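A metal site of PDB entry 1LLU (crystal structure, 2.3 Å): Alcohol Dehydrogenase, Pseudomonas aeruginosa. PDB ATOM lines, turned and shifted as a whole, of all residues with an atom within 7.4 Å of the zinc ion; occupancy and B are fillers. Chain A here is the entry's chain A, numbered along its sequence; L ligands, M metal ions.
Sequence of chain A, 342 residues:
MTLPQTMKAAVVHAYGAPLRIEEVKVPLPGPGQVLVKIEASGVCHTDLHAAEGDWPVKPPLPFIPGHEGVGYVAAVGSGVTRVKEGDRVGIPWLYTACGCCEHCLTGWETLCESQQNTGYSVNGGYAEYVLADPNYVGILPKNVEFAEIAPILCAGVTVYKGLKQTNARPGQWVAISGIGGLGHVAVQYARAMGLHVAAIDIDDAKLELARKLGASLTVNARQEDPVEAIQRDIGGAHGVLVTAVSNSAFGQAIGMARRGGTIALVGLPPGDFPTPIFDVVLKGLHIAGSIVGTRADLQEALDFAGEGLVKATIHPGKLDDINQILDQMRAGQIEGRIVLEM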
ATOM      1  N   GLY A  42       0.182   0.305  25.191  1.00  0.00           N
ATOM      2  CA  GLY A  42       1.345   0.071  24.357  1.00  0.00           C
ATOM      3  C   GLY A  42       1.185  -1.042  23.342  1.00  0.00           C
ATOM      4  O   GLY A  42       0.538  -2.060  23.591  1.00  0.00           O
ATOM      5  N   VAL A  43       1.785  -0.847  22.170  1.00  0.00           N
ATOM      6  CA  VAL A  43       1.717  -1.852  21.107  1.00  0.00           C
ATOM      7  C   VAL A  43       2.986  -2.713  21.159  1.00  0.00           C
ATOM      8  O   VAL A  43       4.089  -2.225  20.897  1.00  0.00           O
ATOM      9  CB  VAL A  43       1.568  -1.175  19.724  1.00  0.00           C
ATOM     10  CG1 VAL A  43       1.550  -2.236  18.623  1.00  0.00           C
ATOM     11  CG2 VAL A  43       0.281  -0.337  19.691  1.00  0.00           C
ATOM     12  N   CYS A  44       2.828  -3.987  21.510  1.00  0.00           N
ATOM     13  CA  CYS A  44       3.934  -4.938  21.608  1.00  0.00           C
ATOM     14  C   CYS A  44       3.945  -5.890  20.401  1.00  0.00           C
ATOM     15  O   CYS A  44       2.895  -6.252  19.865  1.00  0.00           O
ATOM     16  CB  CYS A  44       3.812  -5.732  22.901  1.00  0.00           C
ATOM     17  SG  CYS A  44       5.189  -6.854  23.190  1.00  0.00           S
ATOM     18  N   HIS A  45       5.141  -6.300  19.965  1.00  0.00           N
ATOM     19  CA  HIS A  45       5.252  -7.181  18.817  1.00  0.00           C
ATOM     20  C   HIS A  45       4.559  -8.502  19.060  1.00  0.00           C
ATOM     21  O   HIS A  45       4.204  -9.208  18.124  1.00  0.00           O
ATOM     22  CB  HIS A  45       6.717  -7.424  18.465  1.00  0.00           C
ATOM     23  CG  HIS A  45       6.936  -7.800  17.031  1.00  0.00           C
ATOM     24  ND1 HIS A  45       7.614  -6.989  16.144  1.00  0.00           N
ATOM     25  CD2 HIS A  45       6.606  -8.912  16.339  1.00  0.00           C
ATOM     26  CE1 HIS A  45       7.679  -7.579  14.968  1.00  0.00           C
ATOM     27  NE2 HIS A  45       7.080  -8.756  15.062  1.00  0.00           N
ATOM     28  N   THR A  46       4.375  -8.846  20.335  1.00  0.00           N
ATOM     29  CA  THR A  46       3.684 -10.074  20.694  1.00  0.00           C
ATOM     30  C   THR A  46       2.260  -9.989  20.130  1.00  0.00           C
ATOM     31  O   THR A  46       1.667 -11.016  19.792  1.00  0.00           O
ATOM     32  CB  THR A  46       3.619 -10.260  22.232  1.00  0.00           C
ATOM     33  OG1 THR A  46       4.840 -10.879  22.685  1.00  0.00           O
ATOM     34  CG2 THR A  46       2.453 -11.142  22.644  1.00  0.00           C
ATOM     35  N   ASP A  47       1.724  -8.773  20.032  1.00  0.00           N
ATOM     36  CA  ASP A  47       0.376  -8.556  19.501  1.00  0.00           C
ATOM     37  C   ASP A  47       0.334  -8.971  18.021  1.00  0.00           C
ATOM     38  O   ASP A  47      -0.697  -9.426  17.538  1.00  0.00           O
ATOM     39  CB  ASP A  47      -0.038  -7.088  19.632  1.00  0.00           C
ATOM     40  CG  ASP A  47       0.027  -6.579  21.066  1.00  0.00           C
ATOM     41  OD1 ASP A  47      -0.248  -7.366  21.998  1.00  0.00           O
ATOM     42  OD2 ASP A  47       0.333  -5.386  21.273  1.00  0.00           O
ATOM     43  N   TRP A  55       2.432 -18.544  16.891  1.00  0.00           N
ATOM     44  CA  TRP A  55       2.843 -19.506  17.907  1.00  0.00           C
ATOM     45  C   TRP A  55       2.149 -20.864  17.956  1.00  0.00           C
ATOM     46  O   TRP A  55       1.071 -21.046  17.413  1.00  0.00           O
ATOM     47  CB  TRP A  55       2.787 -18.839  19.289  1.00  0.00           C
ATOM     48  CG  TRP A  55       3.655 -17.583  19.392  1.00  0.00           C
ATOM     49  CD1 TRP A  55       4.701 -17.232  18.583  1.00  0.00           C
ATOM     50  CD2 TRP A  55       3.556 -16.540  20.379  1.00  0.00           C
ATOM     51  NE1 TRP A  55       5.262 -16.042  19.004  1.00  0.00           N
ATOM     52  CE2 TRP A  55       4.577 -15.603  20.101  1.00  0.00           C
ATOM     53  CE3 TRP A  55       2.701 -16.320  21.474  1.00  0.00           C
ATOM     54  CZ2 TRP A  55       4.771 -14.453  20.885  1.00  0.00           C
ATOM     55  CZ3 TRP A  55       2.905 -15.169  22.257  1.00  0.00           C
ATOM     56  CH2 TRP A  55       3.924 -14.251  21.947  1.00  0.00           C
ATOM     57  N   HIS A  67      -1.377  -5.980  26.187  1.00  0.00           N
ATOM     58  CA  HIS A  67      -0.956  -6.284  27.556  1.00  0.00           C
ATOM     59  C   HIS A  67       0.010  -5.224  28.103  1.00  0.00           C
ATOM     60  O   HIS A  67       0.859  -5.513  28.942  1.00  0.00           O
ATOM     61  CB  HIS A  67      -0.302  -7.675  27.635  1.00  0.00           C
ATOM     62  CG  HIS A  67       0.655  -7.940  26.531  1.00  0.00           C
ATOM     63  ND1 HIS A  67       0.249  -8.407  25.293  1.00  0.00           N
ATOM     64  CD2 HIS A  67       1.982  -7.704  26.439  1.00  0.00           C
ATOM     65  CE1 HIS A  67       1.293  -8.437  24.480  1.00  0.00           C
ATOM     66  NE2 HIS A  67       2.348  -8.013  25.150  1.00  0.00           N
ATOM     67  N   GLU A  68      -0.150  -4.004  27.609  1.00  0.00           N
ATOM     68  CA  GLU A  68       0.615  -2.847  28.064  1.00  0.00           C
ATOM     69  C   GLU A  68      -0.427  -1.755  28.293  1.00  0.00           C
ATOM     70  O   GLU A  68      -0.153  -0.559  28.140  1.00  0.00           O
ATOM     71  CB  GLU A  68       1.663  -2.421  27.029  1.00  0.00           C
ATOM     72  CG  GLU A  68       2.889  -3.337  26.990  1.00  0.00           C
ATOM     73  CD  GLU A  68       4.088  -2.743  26.257  1.00  0.00           C
ATOM     74  OE1 GLU A  68       3.922  -1.766  25.486  1.00  0.00           O
ATOM     75  OE2 GLU A  68       5.218  -3.268  26.440  1.00  0.00           O
ATOM     76  N   TRP A  93       1.176  -8.834  30.648  1.00  0.00           N
ATOM     77  CA  TRP A  93       1.010 -10.143  30.023  1.00  0.00           C
ATOM     78  C   TRP A  93       0.542 -11.175  31.042  1.00  0.00           C
ATOM     79  O   TRP A  93      -0.371 -11.949  30.761  1.00  0.00           O
ATOM     80  CB  TRP A  93       2.314 -10.583  29.357  1.00  0.00           C
ATOM     81  CG  TRP A  93       2.287 -11.992  28.807  1.00  0.00           C
ATOM     82  CD1 TRP A  93       2.916 -13.094  29.348  1.00  0.00           C
ATOM     83  CD2 TRP A  93       1.690 -12.428  27.573  1.00  0.00           C
ATOM     84  NE1 TRP A  93       2.746 -14.180  28.516  1.00  0.00           N
ATOM     85  CE2 TRP A  93       1.998 -13.809  27.424  1.00  0.00           C
ATOM     86  CE3 TRP A  93       0.935 -11.793  26.578  1.00  0.00           C
ATOM     87  CZ2 TRP A  93       1.574 -14.566  26.319  1.00  0.00           C
ATOM     88  CZ3 TRP A  93       0.501 -12.551  25.474  1.00  0.00           C
ATOM     89  CH2 TRP A  93       0.831 -13.923  25.354  1.00  0.00           C
ATOM     90  N   LEU A 153       5.090  -1.975  31.331  1.00  0.00           N
ATOM     91  CA  LEU A 153       4.222  -3.108  31.657  1.00  0.00           C
ATOM     92  C   LEU A 153       4.643  -4.398  30.965  1.00  0.00           C
ATOM     93  O   LEU A 153       4.240  -5.487  31.383  1.00  0.00           O
ATOM     94  CB  LEU A 153       2.762  -2.780  31.342  1.00  0.00           C
ATOM     95  CG  LEU A 153       1.987  -2.088  32.471  1.00  0.00           C
ATOM     96  CD1 LEU A 153       1.795  -3.066  33.626  1.00  0.00           C
ATOM     97  CD2 LEU A 153       2.738  -0.841  32.933  1.00  0.00           C
ATOM     98  N   CYS A 154       5.423  -4.292  29.896  1.00  0.00           N
ATOM     99  CA  CYS A 154       5.900  -5.489  29.206  1.00  0.00           C
ATOM    100  C   CYS A 154       7.326  -5.362  28.699  1.00  0.00           C
ATOM    101  O   CYS A 154       8.201  -6.132  29.094  1.00  0.00           O
ATOM    102  CB  CYS A 154       4.994  -5.873  28.056  1.00  0.00           C
ATOM    103  SG  CYS A 154       5.381  -7.545  27.502  1.00  0.00           S
ATOM    104  N   ALA A 155       7.576  -4.408  27.809  1.00  0.00           N
ATOM    105  CA  ALA A 155       8.906  -4.213  27.263  1.00  0.00           C
ATOM    106  C   ALA A 155       9.919  -4.002  28.385  1.00  0.00           C
ATOM    107  O   ALA A 155      10.992  -4.607  28.386  1.00  0.00           O
ATOM    108  CB  ALA A 155       8.910  -3.016  26.315  1.00  0.00           C
ATOM    109  N   THR A 158      10.142  -7.250  31.045  1.00  0.00           N
ATOM    110  CA  THR A 158      10.730  -8.347  30.293  1.00  0.00           C
ATOM    111  C   THR A 158      12.228  -8.200  30.134  1.00  0.00           C
ATOM    112  O   THR A 158      13.017  -9.064  30.529  1.00  0.00           O
ATOM    113  CB  THR A 158      10.113  -8.401  28.884  1.00  0.00           C
ATOM    114  OG1 THR A 158       8.708  -8.661  28.990  1.00  0.00           O
ATOM    115  CG2 THR A 158      10.796  -9.470  28.068  1.00  0.00           C
ATOM    116  N   LEU A 182      11.375  -3.422  23.064  1.00  0.00           N
ATOM    117  CA  LEU A 182      12.067  -4.048  24.184  1.00  0.00           C
ATOM    118  C   LEU A 182      13.514  -3.588  24.269  1.00  0.00           C
ATOM    119  O   LEU A 182      13.993  -3.196  25.327  1.00  0.00           O
ATOM    120  CB  LEU A 182      12.060  -5.573  24.027  1.00  0.00           C
ATOM    121  CG  LEU A 182      11.067  -6.412  24.822  1.00  0.00           C
ATOM    122  CD1 LEU A 182       9.630  -6.029  24.438  1.00  0.00           C
ATOM    123  CD2 LEU A 182      11.365  -7.897  24.577  1.00  0.00           C
ATOM    124  N   VAL A 292       8.577 -12.421  30.235  1.00  0.00           N
ATOM    125  CA  VAL A 292       8.119 -11.213  30.914  1.00  0.00           C
ATOM    126  C   VAL A 292       8.752 -11.116  32.295  1.00  0.00           C
ATOM    127  O   VAL A 292       9.963 -11.293  32.435  1.00  0.00           O
ATOM    128  CB  VAL A 292       6.538 -11.159  31.011  1.00  0.00           C
ATOM    129  CG1 VAL A 292       5.934 -11.062  29.611  1.00  0.00           C
ATOM    130  CG2 VAL A 292       5.980 -12.404  31.711  1.00  0.00           C
ATOM    131  N   ARG A 337       8.653   2.704  20.862  1.00  0.00           N
ATOM    132  CA  ARG A 337       7.308   2.159  21.066  1.00  0.00           C
ATOM    133  C   ARG A 337       6.209   3.125  20.598  1.00  0.00           C
ATOM    134  O   ARG A 337       6.381   4.336  20.603  1.00  0.00           O
ATOM    135  CB  ARG A 337       7.126   1.860  22.576  1.00  0.00           C
ATOM    136  CG  ARG A 337       6.078   0.814  22.969  1.00  0.00           C
ATOM    137  CD  ARG A 337       6.429  -0.528  22.419  1.00  0.00           C
ATOM    138  NE  ARG A 337       6.107  -1.644  23.302  1.00  0.00           N
ATOM    139  CZ  ARG A 337       6.536  -2.886  23.095  1.00  0.00           C
ATOM    140  NH1 ARG A 337       7.284  -3.152  22.024  1.00  0.00           N
ATOM    141  NH2 ARG A 337       6.255  -3.848  23.955  1.00  0.00           N
HETATM  142  C1  LIG L   1       5.255 -12.485  25.990  1.00  0.00           C
HETATM  143  O1  LIG L   1       4.831 -13.012  24.729  1.00  0.00           O
HETATM  144  C2  LIG L   1       4.537 -11.210  26.249  1.00  0.00           C
HETATM  145  O2  LIG L   1       4.757 -10.172  25.266  1.00  0.00           O
HETATM  146  P1  LG2 L   2      10.016  -4.592  17.747  1.00  0.00           P
HETATM  147  O1  LG2 L   2       9.710  -3.233  18.235  1.00  0.00           O
HETATM  148  O2  LG2 L   2       9.417  -5.065  16.470  1.00  0.00           O
HETATM  149  O3  LG2 L   2      11.592  -4.670  17.709  1.00  0.00           O
HETATM  150  C1  LG2 L   2      12.336  -5.805  17.176  1.00  0.00           C
HETATM  151  C2  LG2 L   2      13.679  -5.248  16.782  1.00  0.00           C
HETATM  152  O4  LG2 L   2      14.450  -6.370  16.218  1.00  0.00           O
HETATM  153  C3  LG2 L   2      13.636  -4.171  15.648  1.00  0.00           C
HETATM  154  O5  LG2 L   2      14.248  -2.942  16.128  1.00  0.00           O
HETATM  155  C4  LG2 L   2      14.365  -4.793  14.476  1.00  0.00           C
HETATM  156  O6  LG2 L   2      14.989  -3.952  13.555  1.00  0.00           O
HETATM  157  C5  LG2 L   2      15.272  -5.795  15.216  1.00  0.00           C
HETATM  158  N1  LG2 L   2      15.702  -6.872  14.346  1.00  0.00           N
HETATM  159  C6  LG2 L   2      15.063  -7.615  13.336  1.00  0.00           C
HETATM  160  N2  LG2 L   2      15.844  -8.527  12.775  1.00  0.00           N
HETATM  161  C7  LG2 L   2      17.041  -8.443  13.375  1.00  0.00           C
HETATM  162  C8  LG2 L   2      18.299  -9.169  13.206  1.00  0.00           C
HETATM  163  N3  LG2 L   2      18.440 -10.126  12.302  1.00  0.00           N
HETATM  164  N4  LG2 L   2      19.326  -8.769  14.048  1.00  0.00           N
HETATM  165  C9  LG2 L   2      19.237  -7.801  14.979  1.00  0.00           C
HETATM  166  N5  LG2 L   2      18.061  -7.065  15.193  1.00  0.00           N
HETATM  167  C10 LG2 L   2      16.993  -7.418  14.367  1.00  0.00           C
HETATM  168  O7  LG2 L   2       9.615  -5.666  18.849  1.00  0.00           O
HETATM  169  P2  LG2 L   2       9.316  -5.525  20.444  1.00  0.00           P
HETATM  170  O8  LG2 L   2      10.410  -5.187  21.358  1.00  0.00           O
HETATM  171  O9  LG2 L   2       8.061  -6.201  20.865  1.00  0.00           O
HETATM  172  O10 LG2 L   2      10.090  -6.986  20.451  1.00  0.00           O
HETATM  173  C11 LG2 L   2       9.621  -8.087  19.648  1.00  0.00           C
HETATM  174  C12 LG2 L   2       9.869  -9.453  20.147  1.00  0.00           C
HETATM  175  O11 LG2 L   2       9.809  -9.567  21.660  1.00  0.00           O
HETATM  176  C13 LG2 L   2       8.738 -10.401  19.618  1.00  0.00           C
HETATM  177  O12 LG2 L   2       9.243 -11.663  19.173  1.00  0.00           O
HETATM  178  C14 LG2 L   2       7.837 -10.513  20.845  1.00  0.00           C
HETATM  179  O13 LG2 L   2       6.859 -11.497  20.806  1.00  0.00           O
HETATM  180  C15 LG2 L   2       8.898 -10.652  21.982  1.00  0.00           C
HETATM  181  N6  LG2 L   2       8.244 -10.549  23.307  1.00  0.00           N
HETATM  182  C16 LG2 L   2       8.721 -11.486  24.280  1.00  0.00           C
HETATM  183  C17 LG2 L   2       8.644 -11.286  25.603  1.00  0.00           C
HETATM  184  C18 LG2 L   2       9.146 -12.332  26.568  1.00  0.00           C
HETATM  185  O14 LG2 L   2       8.685 -12.309  27.724  1.00  0.00           O
HETATM  186  N7  LG2 L   2      10.019 -13.261  26.180  1.00  0.00           N
HETATM  187  C19 LG2 L   2       8.036  -9.998  26.187  1.00  0.00           C
HETATM  188  C20 LG2 L   2       8.150  -8.873  25.187  1.00  0.00           C
HETATM  189  C21 LG2 L   2       7.979  -9.190  23.812  1.00  0.00           C
HETATM  190 ZN    ZN M   1       4.578  -7.999  25.206  1.00  0.00          ZN
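Residues that only touch the zinc ion: Thr 46. Of the 17 residues printed, 4 come within 4 Å of the zinc ion. The nearest printed residue that does not touch the zinc ion is Arg 337 (4.6 Å).
N of Thr 46 lies close to SG of Cys 44 (3.6 Å). The side-chain hydroxyl (OG1) of Thr 158 lies within hydrogen-bond range of the backbone carbonyl oxygen (O) of Cys 154 (2.6 Å). SG of Cys 44 lies close to NH2 of Arg 337. N of Cys 44 sits at hydrogen-bond distance from OD2 of Asp 47, at 2.9 Å. The side-chain carboxylate (OD1) of Asp 47 lies close to a ring nitrogen (ND1) of His 67 (3.5 Å).
The side-chain sulfur of Cys 44 lies close to an oxygen (O9) of LG2 L2 (3.8 Å). An oxygen (O9) of LG2 L2 lies close to the backbone NH (N) of His 45, at 3.1 Å. O14 of LG2 L2 is in hydrogen-bond range of N of Val 292, at 2.5 Å. The backbone NH of Leu 182 is in hydrogen-bond range of an oxygen (O8) of LG2 L2, 2.6 Å away. ND1 of His 45 sits at hydrogen-bond distance from O2 of LG2 L2 (2.7 Å). An oxygen (O13) of LG2 L2 is in hydrogen-bond range of the side-chain hydroxyl (OG1) of Thr 46 (2.8 Å). An oxygen (O9) of LG2 L2 lies within salt-bridge range of the guanidinium group of Arg 337 (3.4 Å).
The zinc ion is bound by O2 of LIG L1, NE2 of His 67, SG of Cys 44 and SG of Cys 154. The zinc ion has four donor atoms within binding distance.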
